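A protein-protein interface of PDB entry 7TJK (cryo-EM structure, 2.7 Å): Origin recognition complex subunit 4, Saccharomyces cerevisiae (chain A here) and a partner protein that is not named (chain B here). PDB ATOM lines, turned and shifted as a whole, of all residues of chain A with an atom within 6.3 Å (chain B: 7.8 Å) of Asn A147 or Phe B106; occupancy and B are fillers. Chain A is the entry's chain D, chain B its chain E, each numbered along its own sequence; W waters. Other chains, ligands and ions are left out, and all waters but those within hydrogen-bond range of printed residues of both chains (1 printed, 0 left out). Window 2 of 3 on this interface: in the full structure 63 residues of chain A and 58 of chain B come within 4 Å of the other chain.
The backbone carbonyl oxygen (O) of Asn A147 sits at hydrogen-bond distance from the side-chain hydroxyl (OG1) of Thr A151 (3.2 Å).
Among the printed residues, merely in contact across the chains: Ile A139 with Pro B105, Ile A139 with Phe B106, Ile A139 with Leu B155, His A140 with Phe B106, Thr A144 with Phe B106 and Asn A147 with Phe B106.
Printed residues of chain A within 4 Å of Phe B106: Ile A139, His A140, Thr A144 and Asn A147.
No residue of chain B comes within 4 Å of Gly A148.
Of the printed residues of chain A, Leu B155 touches Ile A139 (3.8 Å).
Of the printed residues of chain B, His A140 touches Phe B106 (3.96 Å).
Printed residues of chain A within 4 Å of Pro B105: Ile A139 (3.8 Å).
Printed residues of chain B within 4 Å of Ile A139: Pro B105, Phe B106 and Leu B155.
Of the printed residues of chain B, Thr A144 touches Phe B106.
The nearest residue of chain A that does not touch Phe B106 is Gly A148 (4.5 Å).
The nearest printed residue of chain B that does not touch Ile A139 is Val B109 (4.6 Å).
Printed residues of chain A that touch a printed residue of chain B: Ile A139, His A140, Thr A144 and Asn A147.
Hydrophobic or aromatic side chains of chain A that line the printed part of chain B: Ile A139 and His A140.
Printed residues of chain B that touch a printed residue of chain A: Pro B105, Phe B106 and Leu B155.
Water W1 lies within hydrogen-bond range of O of Ile A139 (2.5 Å) and N of Phe B106 (3.4 Å).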
ATOM      1  N   ILE A 139      -5.502   4.310 -14.745  1.00  0.00           N
ATOM      2  CA  ILE A 139      -6.705   5.006 -15.194  1.00  0.00           C
ATOM      3  C   ILE A 139      -7.183   4.460 -16.534  1.00  0.00           C
ATOM      4  O   ILE A 139      -8.367   4.149 -16.706  1.00  0.00           O
ATOM      5  CB  ILE A 139      -6.471   6.534 -15.247  1.00  0.00           C
ATOM      6  CG1 ILE A 139      -6.251   7.140 -13.848  1.00  0.00           C
ATOM      7  CG2 ILE A 139      -7.613   7.250 -15.956  1.00  0.00           C
ATOM      8  CD1 ILE A 139      -4.816   7.230 -13.358  1.00  0.00           C
ATOM      9  N   HIS A 140      -6.278   4.306 -17.494  1.00  0.00           N
ATOM     10  CA  HIS A 140      -6.657   3.890 -18.837  1.00  0.00           C
ATOM     11  C   HIS A 140      -6.629   2.372 -18.950  1.00  0.00           C
ATOM     12  O   HIS A 140      -5.659   1.728 -18.538  1.00  0.00           O
ATOM     13  CB  HIS A 140      -5.728   4.502 -19.885  1.00  0.00           C
ATOM     14  CG  HIS A 140      -5.839   5.990 -19.999  1.00  0.00           C
ATOM     15  ND1 HIS A 140      -4.960   6.850 -19.379  1.00  0.00           N
ATOM     16  CD2 HIS A 140      -6.723   6.770 -20.663  1.00  0.00           C
ATOM     17  CE1 HIS A 140      -5.297   8.096 -19.656  1.00  0.00           C
ATOM     18  NE2 HIS A 140      -6.364   8.075 -20.432  1.00  0.00           N
ATOM     19  N   GLN A 143      -8.990  -0.426 -23.863  1.00  0.00           N
ATOM     20  CA  GLN A 143      -9.927   0.116 -24.831  1.00  0.00           C
ATOM     21  C   GLN A 143     -10.155   1.611 -24.655  1.00  0.00           C
ATOM     22  O   GLN A 143     -10.428   2.304 -25.641  1.00  0.00           O
ATOM     23  CB  GLN A 143     -11.261  -0.628 -24.737  1.00  0.00           C
ATOM     24  CG  GLN A 143     -11.144  -2.108 -25.086  1.00  0.00           C
ATOM     25  CD  GLN A 143     -10.771  -2.357 -26.534  1.00  0.00           C
ATOM     26  OE1 GLN A 143     -11.231  -1.665 -27.436  1.00  0.00           O
ATOM     27  NE2 GLN A 143      -9.926  -3.356 -26.759  1.00  0.00           N
ATOM     28  N   THR A 144     -10.043   2.122 -23.432  1.00  0.00           N
ATOM     29  CA  THR A 144     -10.225   3.539 -23.153  1.00  0.00           C
ATOM     30  C   THR A 144      -8.981   4.370 -23.443  1.00  0.00           C
ATOM     31  O   THR A 144      -9.073   5.604 -23.502  1.00  0.00           O
ATOM     32  CB  THR A 144     -10.637   3.728 -21.693  1.00  0.00           C
ATOM     33  OG1 THR A 144      -9.604   3.238 -20.831  1.00  0.00           O
ATOM     34  CG2 THR A 144     -11.924   2.968 -21.414  1.00  0.00           C
ATOM     35  N   ALA A 145      -7.828   3.722 -23.629  1.00  0.00           N
ATOM     36  CA  ALA A 145      -6.613   4.444 -23.982  1.00  0.00           C
ATOM     37  C   ALA A 145      -6.701   5.042 -25.378  1.00  0.00           C
ATOM     38  O   ALA A 145      -6.080   6.074 -25.638  1.00  0.00           O
ATOM     39  CB  ALA A 145      -5.398   3.522 -23.875  1.00  0.00           C
ATOM     40  N   ILE A 146      -7.473   4.423 -26.275  1.00  0.00           N
ATOM     41  CA  ILE A 146      -7.680   4.976 -27.611  1.00  0.00           C
ATOM     42  C   ILE A 146      -8.436   6.300 -27.532  1.00  0.00           C
ATOM     43  O   ILE A 146      -8.059   7.289 -28.173  1.00  0.00           O
ATOM     44  CB  ILE A 146      -8.410   3.951 -28.499  1.00  0.00           C
ATOM     45  CG1 ILE A 146      -7.536   2.713 -28.697  1.00  0.00           C
ATOM     46  CG2 ILE A 146      -8.777   4.550 -29.850  1.00  0.00           C
ATOM     47  CD1 ILE A 146      -8.312   1.475 -29.075  1.00  0.00           C
ATOM     48  N   ASN A 147      -9.493   6.345 -26.716  1.00  0.00           N
ATOM     49  CA  ASN A 147     -10.230   7.589 -26.514  1.00  0.00           C
ATOM     50  C   ASN A 147      -9.393   8.631 -25.783  1.00  0.00           C
ATOM     51  O   ASN A 147      -9.493   9.824 -26.094  1.00  0.00           O
ATOM     52  CB  ASN A 147     -11.527   7.321 -25.753  1.00  0.00           C
ATOM     53  CG  ASN A 147     -12.538   6.546 -26.574  1.00  0.00           C
ATOM     54  OD1 ASN A 147     -13.014   5.492 -26.156  1.00  0.00           O
ATOM     55  ND2 ASN A 147     -12.871   7.064 -27.750  1.00  0.00           N
ATOM     56  N   GLY A 148      -8.565   8.201 -24.824  1.00  0.00           N
ATOM     57  CA  GLY A 148      -7.670   9.134 -24.153  1.00  0.00           C
ATOM     58  C   GLY A 148      -6.651   9.755 -25.092  1.00  0.00           C
ATOM     59  O   GLY A 148      -6.442  10.974 -25.074  1.00  0.00           O
ATOM     60  N   ILE A 149      -6.045   8.929 -25.957  1.00  0.00           N
ATOM     61  CA  ILE A 149      -5.103   9.407 -26.968  1.00  0.00           C
ATOM     62  C   ILE A 149      -5.793  10.358 -27.935  1.00  0.00           C
ATOM     63  O   ILE A 149      -5.250  11.418 -28.271  1.00  0.00           O
ATOM     64  CB  ILE A 149      -4.463   8.212 -27.706  1.00  0.00           C
ATOM     65  CG1 ILE A 149      -3.421   7.512 -26.838  1.00  0.00           C
ATOM     66  CG2 ILE A 149      -3.826   8.628 -29.030  1.00  0.00           C
ATOM     67  CD1 ILE A 149      -3.070   6.132 -27.345  1.00  0.00           C
ATOM     68  N   ALA A 150      -7.019  10.020 -28.354  1.00  0.00           N
ATOM     69  CA  ALA A 150      -7.748  10.846 -29.313  1.00  0.00           C
ATOM     70  C   ALA A 150      -8.085  12.220 -28.745  1.00  0.00           C
ATOM     71  O   ALA A 150      -7.734  13.238 -29.355  1.00  0.00           O
ATOM     72  CB  ALA A 150      -9.023  10.131 -29.750  1.00  0.00           C
ATOM     73  N   THR A 151      -8.701  12.268 -27.555  1.00  0.00           N
ATOM     74  CA  THR A 151      -9.089  13.553 -26.971  1.00  0.00           C
ATOM     75  C   THR A 151      -7.873  14.382 -26.574  1.00  0.00           C
ATOM     76  O   THR A 151      -7.900  15.617 -26.688  1.00  0.00           O
ATOM     77  CB  THR A 151     -10.027  13.351 -25.776  1.00  0.00           C
ATOM     78  OG1 THR A 151      -9.335  12.695 -24.704  1.00  0.00           O
ATOM     79  CG2 THR A 151     -11.267  12.555 -26.174  1.00  0.00           C
ATOM     80  N   GLN A 152      -6.782  13.727 -26.152  1.00  0.00           N
ATOM     81  CA  GLN A 152      -5.542  14.462 -25.944  1.00  0.00           C
ATOM     82  C   GLN A 152      -4.976  14.998 -27.252  1.00  0.00           C
ATOM     83  O   GLN A 152      -4.372  16.074 -27.257  1.00  0.00           O
ATOM     84  CB  GLN A 152      -4.520  13.591 -25.218  1.00  0.00           C
ATOM     85  CG  GLN A 152      -4.767  13.509 -23.722  1.00  0.00           C
ATOM     86  CD  GLN A 152      -3.781  12.614 -23.019  1.00  0.00           C
ATOM     87  OE1 GLN A 152      -2.657  13.019 -22.735  1.00  0.00           O
ATOM     88  NE2 GLN A 152      -4.195  11.387 -22.728  1.00  0.00           N
ATOM     89  N   SER A 176     -11.565  12.335 -32.295  1.00  0.00           N
ATOM     90  CA  SER A 176     -12.238  11.676 -31.184  1.00  0.00           C
ATOM     91  C   SER A 176     -13.735  11.498 -31.395  1.00  0.00           C
ATOM     92  O   SER A 176     -14.427  11.067 -30.469  1.00  0.00           O
ATOM     93  CB  SER A 176     -12.003  12.455 -29.885  1.00  0.00           C
ATOM     94  OG  SER A 176     -12.532  13.765 -29.970  1.00  0.00           O
ATOM     95  N   GLY A 178     -17.043   9.664 -33.168  1.00  0.00           N
ATOM     96  CA  GLY A 178     -17.450   8.407 -33.760  1.00  0.00           C
ATOM     97  C   GLY A 178     -17.151   7.226 -32.857  1.00  0.00           C
ATOM     98  O   GLY A 178     -16.699   7.368 -31.718  1.00  0.00           O
ATOM     99  N   SER A 179     -17.399   6.036 -33.401  1.00  0.00           N
ATOM    100  CA  SER A 179     -17.205   4.800 -32.658  1.00  0.00           C
ATOM    101  C   SER A 179     -15.716   4.499 -32.491  1.00  0.00           C
ATOM    102  O   SER A 179     -14.847   5.179 -33.042  1.00  0.00           O
ATOM    103  CB  SER A 179     -17.904   3.636 -33.358  1.00  0.00           C
ATOM    104  OG  SER A 179     -17.270   3.318 -34.584  1.00  0.00           O
ATOM    105  N   LEU A 180     -15.436   3.451 -31.708  1.00  0.00           N
ATOM    106  CA  LEU A 180     -14.064   3.079 -31.372  1.00  0.00           C
ATOM    107  C   LEU A 180     -13.268   2.642 -32.597  1.00  0.00           C
ATOM    108  O   LEU A 180     -12.076   2.959 -32.701  1.00  0.00           O
ATOM    109  CB  LEU A 180     -14.076   1.968 -30.326  1.00  0.00           C
ATOM    110  CG  LEU A 180     -12.923   1.922 -29.328  1.00  0.00           C
ATOM    111  CD1 LEU A 180     -12.748   3.259 -28.638  1.00  0.00           C
ATOM    112  CD2 LEU A 180     -13.186   0.829 -28.316  1.00  0.00           C
ATOM    113  N   VAL A 183     -12.481   5.891 -34.472  1.00  0.00           N
ATOM    114  CA  VAL A 183     -11.494   6.691 -33.749  1.00  0.00           C
ATOM    115  C   VAL A 183     -10.101   6.081 -33.877  1.00  0.00           C
ATOM    116  O   VAL A 183      -9.121   6.794 -34.134  1.00  0.00           O
ATOM    117  CB  VAL A 183     -11.935   6.852 -32.281  1.00  0.00           C
ATOM    118  CG1 VAL A 183     -10.791   7.306 -31.398  1.00  0.00           C
ATOM    119  CG2 VAL A 183     -13.077   7.848 -32.189  1.00  0.00           C
ATOM    120  N   ILE A 187      -6.869   7.663 -35.780  1.00  0.00           N
ATOM    121  CA  ILE A 187      -5.566   7.764 -35.118  1.00  0.00           C
ATOM    122  C   ILE A 187      -4.479   7.121 -35.978  1.00  0.00           C
ATOM    123  O   ILE A 187      -3.383   7.678 -36.139  1.00  0.00           O
ATOM    124  CB  ILE A 187      -5.636   7.137 -33.709  1.00  0.00           C
ATOM    125  CG1 ILE A 187      -6.384   8.058 -32.747  1.00  0.00           C
ATOM    126  CG2 ILE A 187      -4.251   6.847 -33.141  1.00  0.00           C
ATOM    127  CD1 ILE A 187      -6.687   7.428 -31.413  1.00  0.00           C
ATOM    128  N   LEU B  74     -17.275   8.504  -8.699  1.00  0.00           N
ATOM    129  CA  LEU B  74     -16.812   9.378  -9.779  1.00  0.00           C
ATOM    130  C   LEU B  74     -17.878  10.397 -10.168  1.00  0.00           C
ATOM    131  O   LEU B  74     -17.573  11.582 -10.378  1.00  0.00           O
ATOM    132  CB  LEU B  74     -16.418   8.554 -11.006  1.00  0.00           C
ATOM    133  CG  LEU B  74     -15.339   7.473 -10.949  1.00  0.00           C
ATOM    134  CD1 LEU B  74     -15.293   6.715 -12.264  1.00  0.00           C
ATOM    135  CD2 LEU B  74     -13.983   8.052 -10.627  1.00  0.00           C
ATOM    136  N   GLN B 101     -22.323  11.752 -17.298  1.00  0.00           N
ATOM    137  CA  GLN B 101     -21.439  11.470 -18.428  1.00  0.00           C
ATOM    138  C   GLN B 101     -20.229  10.639 -18.012  1.00  0.00           C
ATOM    139  O   GLN B 101     -19.548  10.070 -18.870  1.00  0.00           O
ATOM    140  CB  GLN B 101     -20.947  12.771 -19.069  1.00  0.00           C
ATOM    141  CG  GLN B 101     -21.996  13.653 -19.730  1.00  0.00           C
ATOM    142  CD  GLN B 101     -22.693  12.993 -20.900  1.00  0.00           C
ATOM    143  OE1 GLN B 101     -23.870  12.646 -20.817  1.00  0.00           O
ATOM    144  NE2 GLN B 101     -21.972  12.820 -22.000  1.00  0.00           N
ATOM    145  N   VAL B 102     -19.922  10.591 -16.718  1.00  0.00           N
ATOM    146  CA  VAL B 102     -18.731   9.911 -16.220  1.00  0.00           C
ATOM    147  C   VAL B 102     -19.090   8.462 -15.898  1.00  0.00           C
ATOM    148  O   VAL B 102     -19.762   8.191 -14.900  1.00  0.00           O
ATOM    149  CB  VAL B 102     -18.158  10.624 -14.989  1.00  0.00           C
ATOM    150  CG1 VAL B 102     -16.904   9.920 -14.497  1.00  0.00           C
ATOM    151  CG2 VAL B 102     -17.875  12.081 -15.304  1.00  0.00           C
ATOM    152  N   GLU B 103     -18.646   7.527 -16.738  1.00  0.00           N
ATOM    153  CA  GLU B 103     -18.703   6.109 -16.395  1.00  0.00           C
ATOM    154  C   GLU B 103     -17.340   5.477 -16.169  1.00  0.00           C
ATOM    155  O   GLU B 103     -17.283   4.383 -15.600  1.00  0.00           O
ATOM    156  CB  GLU B 103     -19.433   5.289 -17.474  1.00  0.00           C
ATOM    157  CG  GLU B 103     -20.923   5.559 -17.642  1.00  0.00           C
ATOM    158  CD  GLU B 103     -21.223   6.750 -18.518  1.00  0.00           C
ATOM    159  OE1 GLU B 103     -20.269   7.337 -19.060  1.00  0.00           O
ATOM    160  OE2 GLU B 103     -22.413   7.092 -18.677  1.00  0.00           O
ATOM    161  N   GLU B 104     -16.257   6.115 -16.585  1.00  0.00           N
ATOM    162  CA  GLU B 104     -14.898   5.607 -16.509  1.00  0.00           C
ATOM    163  C   GLU B 104     -14.009   6.682 -15.902  1.00  0.00           C
ATOM    164  O   GLU B 104     -14.379   7.861 -15.890  1.00  0.00           O
ATOM    165  CB  GLU B 104     -14.396   5.212 -17.907  1.00  0.00           C
ATOM    166  CG  GLU B 104     -14.994   3.934 -18.477  1.00  0.00           C
ATOM    167  CD  GLU B 104     -14.798   2.728 -17.573  1.00  0.00           C
ATOM    168  OE1 GLU B 104     -13.666   2.202 -17.523  1.00  0.00           O
ATOM    169  OE2 GLU B 104     -15.774   2.290 -16.930  1.00  0.00           O
ATOM    170  N   PRO B 105     -12.854   6.302 -15.333  1.00  0.00           N
ATOM    171  CA  PRO B 105     -11.947   7.320 -14.763  1.00  0.00           C
ATOM    172  C   PRO B 105     -11.385   8.326 -15.761  1.00  0.00           C
ATOM    173  O   PRO B 105     -11.132   9.478 -15.371  1.00  0.00           O
ATOM    174  CB  PRO B 105     -10.833   6.471 -14.138  1.00  0.00           C
ATOM    175  CG  PRO B 105     -11.496   5.201 -13.788  1.00  0.00           C
ATOM    176  CD  PRO B 105     -12.492   4.946 -14.874  1.00  0.00           C
ATOM    177  N   PHE B 106     -11.191   7.951 -17.032  1.00  0.00           N
ATOM    178  CA  PHE B 106     -10.652   8.927 -17.975  1.00  0.00           C
ATOM    179  C   PHE B 106     -11.728   9.944 -18.322  1.00  0.00           C
ATOM    180  O   PHE B 106     -11.419  11.092 -18.652  1.00  0.00           O
ATOM    181  CB  PHE B 106     -10.140   8.253 -19.259  1.00  0.00           C
ATOM    182  CG  PHE B 106     -11.225   7.859 -20.228  1.00  0.00           C
ATOM    183  CD1 PHE B 106     -11.947   6.694 -20.074  1.00  0.00           C
ATOM    184  CD2 PHE B 106     -11.447   8.632 -21.368  1.00  0.00           C
ATOM    185  CE1 PHE B 106     -12.941   6.361 -20.983  1.00  0.00           C
ATOM    186  CE2 PHE B 106     -12.420   8.291 -22.280  1.00  0.00           C
ATOM    187  CZ  PHE B 106     -13.163   7.151 -22.090  1.00  0.00           C
ATOM    188  N   LEU B 107     -12.995   9.527 -18.247  1.00  0.00           N
ATOM    189  CA  LEU B 107     -14.111  10.445 -18.412  1.00  0.00           C
ATOM    190  C   LEU B 107     -14.182  11.433 -17.261  1.00  0.00           C
ATOM    191  O   LEU B 107     -14.540  12.594 -17.472  1.00  0.00           O
ATOM    192  CB  LEU B 107     -15.415   9.660 -18.535  1.00  0.00           C
ATOM    193  CG  LEU B 107     -15.594   8.914 -19.858  1.00  0.00           C
ATOM    194  CD1 LEU B 107     -16.904   8.148 -19.876  1.00  0.00           C
ATOM    195  CD2 LEU B 107     -15.505   9.871 -21.036  1.00  0.00           C
ATOM    196  N   LEU B 108     -13.830  10.995 -16.046  1.00  0.00           N
ATOM    197  CA  LEU B 108     -13.685  11.924 -14.929  1.00  0.00           C
ATOM    198  C   LEU B 108     -12.559  12.916 -15.183  1.00  0.00           C
ATOM    199  O   LEU B 108     -12.709  14.110 -14.896  1.00  0.00           O
ATOM    200  CB  LEU B 108     -13.437  11.168 -13.623  1.00  0.00           C
ATOM    201  CG  LEU B 108     -13.255  12.078 -12.400  1.00  0.00           C
ATOM    202  CD1 LEU B 108     -14.584  12.670 -11.954  1.00  0.00           C
ATOM    203  CD2 LEU B 108     -12.543  11.389 -11.251  1.00  0.00           C
ATOM    204  N   VAL B 109     -11.435  12.439 -15.732  1.00  0.00           N
ATOM    205  CA  VAL B 109     -10.307  13.323 -16.043  1.00  0.00           C
ATOM    206  C   VAL B 109     -10.706  14.359 -17.094  1.00  0.00           C
ATOM    207  O   VAL B 109     -10.435  15.557 -16.945  1.00  0.00           O
ATOM    208  CB  VAL B 109      -9.089  12.490 -16.493  1.00  0.00           C
ATOM    209  CG1 VAL B 109      -7.985  13.376 -17.051  1.00  0.00           C
ATOM    210  CG2 VAL B 109      -8.563  11.663 -15.336  1.00  0.00           C
ATOM    211  N   LYS B 110     -11.405  13.912 -18.141  1.00  0.00           N
ATOM    212  CA  LYS B 110     -11.866  14.807 -19.202  1.00  0.00           C
ATOM    213  C   LYS B 110     -12.901  15.810 -18.695  1.00  0.00           C
ATOM    214  O   LYS B 110     -12.846  16.994 -19.050  1.00  0.00           O
ATOM    215  CB  LYS B 110     -12.438  13.987 -20.357  1.00  0.00           C
ATOM    216  CG  LYS B 110     -12.839  14.810 -21.568  1.00  0.00           C
ATOM    217  CD  LYS B 110     -13.389  13.938 -22.681  1.00  0.00           C
ATOM    218  CE  LYS B 110     -14.773  13.424 -22.342  1.00  0.00           C
ATOM    219  NZ  LYS B 110     -15.759  14.530 -22.216  1.00  0.00           N
ATOM    220  N   THR B 111     -13.841  15.357 -17.858  1.00  0.00           N
ATOM    221  CA  THR B 111     -14.861  16.244 -17.307  1.00  0.00           C
ATOM    222  C   THR B 111     -14.254  17.278 -16.365  1.00  0.00           C
ATOM    223  O   THR B 111     -14.634  18.454 -16.405  1.00  0.00           O
ATOM    224  CB  THR B 111     -15.931  15.423 -16.586  1.00  0.00           C
ATOM    225  OG1 THR B 111     -16.354  14.346 -17.428  1.00  0.00           O
ATOM    226  CG2 THR B 111     -17.134  16.283 -16.243  1.00  0.00           C
ATOM    227  N   LEU B 112     -13.298  16.861 -15.527  1.00  0.00           N
ATOM    228  CA  LEU B 112     -12.612  17.793 -14.638  1.00  0.00           C
ATOM    229  C   LEU B 112     -11.783  18.801 -15.423  1.00  0.00           C
ATOM    230  O   LEU B 112     -11.725  19.977 -15.053  1.00  0.00           O
ATOM    231  CB  LEU B 112     -11.729  17.028 -13.654  1.00  0.00           C
ATOM    232  CG  LEU B 112     -12.394  16.373 -12.441  1.00  0.00           C
ATOM    233  CD1 LEU B 112     -11.363  15.616 -11.623  1.00  0.00           C
ATOM    234  CD2 LEU B 112     -13.116  17.397 -11.579  1.00  0.00           C
ATOM    235  N   HIS B 113     -11.149  18.360 -16.516  1.00  0.00           N
ATOM    236  CA  HIS B 113     -10.403  19.276 -17.375  1.00  0.00           C
ATOM    237  C   HIS B 113     -11.322  20.301 -18.028  1.00  0.00           C
ATOM    238  O   HIS B 113     -11.003  21.496 -18.062  1.00  0.00           O
ATOM    239  CB  HIS B 113      -9.640  18.481 -18.435  1.00  0.00           C
ATOM    240  CG  HIS B 113      -8.910  19.331 -19.428  1.00  0.00           C
ATOM    241  ND1 HIS B 113      -7.626  19.781 -19.221  1.00  0.00           N
ATOM    242  CD2 HIS B 113      -9.280  19.800 -20.644  1.00  0.00           C
ATOM    243  CE1 HIS B 113      -7.238  20.497 -20.261  1.00  0.00           C
ATOM    244  NE2 HIS B 113      -8.224  20.525 -21.138  1.00  0.00           N
ATOM    245  N   LEU B 152      -4.274  10.708 -10.072  1.00  0.00           N
ATOM    246  CA  LEU B 152      -5.288  11.478 -10.787  1.00  0.00           C
ATOM    247  C   LEU B 152      -4.836  12.905 -11.077  1.00  0.00           C
ATOM    248  O   LEU B 152      -5.209  13.470 -12.111  1.00  0.00           O
ATOM    249  CB  LEU B 152      -6.591  11.494  -9.991  1.00  0.00           C
ATOM    250  CG  LEU B 152      -7.831  11.900 -10.783  1.00  0.00           C
ATOM    251  CD1 LEU B 152      -8.281  10.751 -11.669  1.00  0.00           C
ATOM    252  CD2 LEU B 152      -8.944  12.350  -9.859  1.00  0.00           C
ATOM    253  N   LEU B 155      -2.803  13.521 -14.478  1.00  0.00           N
ATOM    254  CA  LEU B 155      -3.524  13.614 -15.742  1.00  0.00           C
ATOM    255  C   LEU B 155      -4.284  14.923 -15.899  1.00  0.00           C
ATOM    256  O   LEU B 155      -4.928  15.129 -16.932  1.00  0.00           O
ATOM    257  CB  LEU B 155      -4.496  12.439 -15.889  1.00  0.00           C
ATOM    258  CG  LEU B 155      -3.902  11.034 -15.813  1.00  0.00           C
ATOM    259  CD1 LEU B 155      -4.960   9.996 -16.138  1.00  0.00           C
ATOM    260  CD2 LEU B 155      -2.708  10.900 -16.741  1.00  0.00           C
HETATM  261  O   HOH W   1     -10.549   4.732 -17.790  1.00  0.00           O
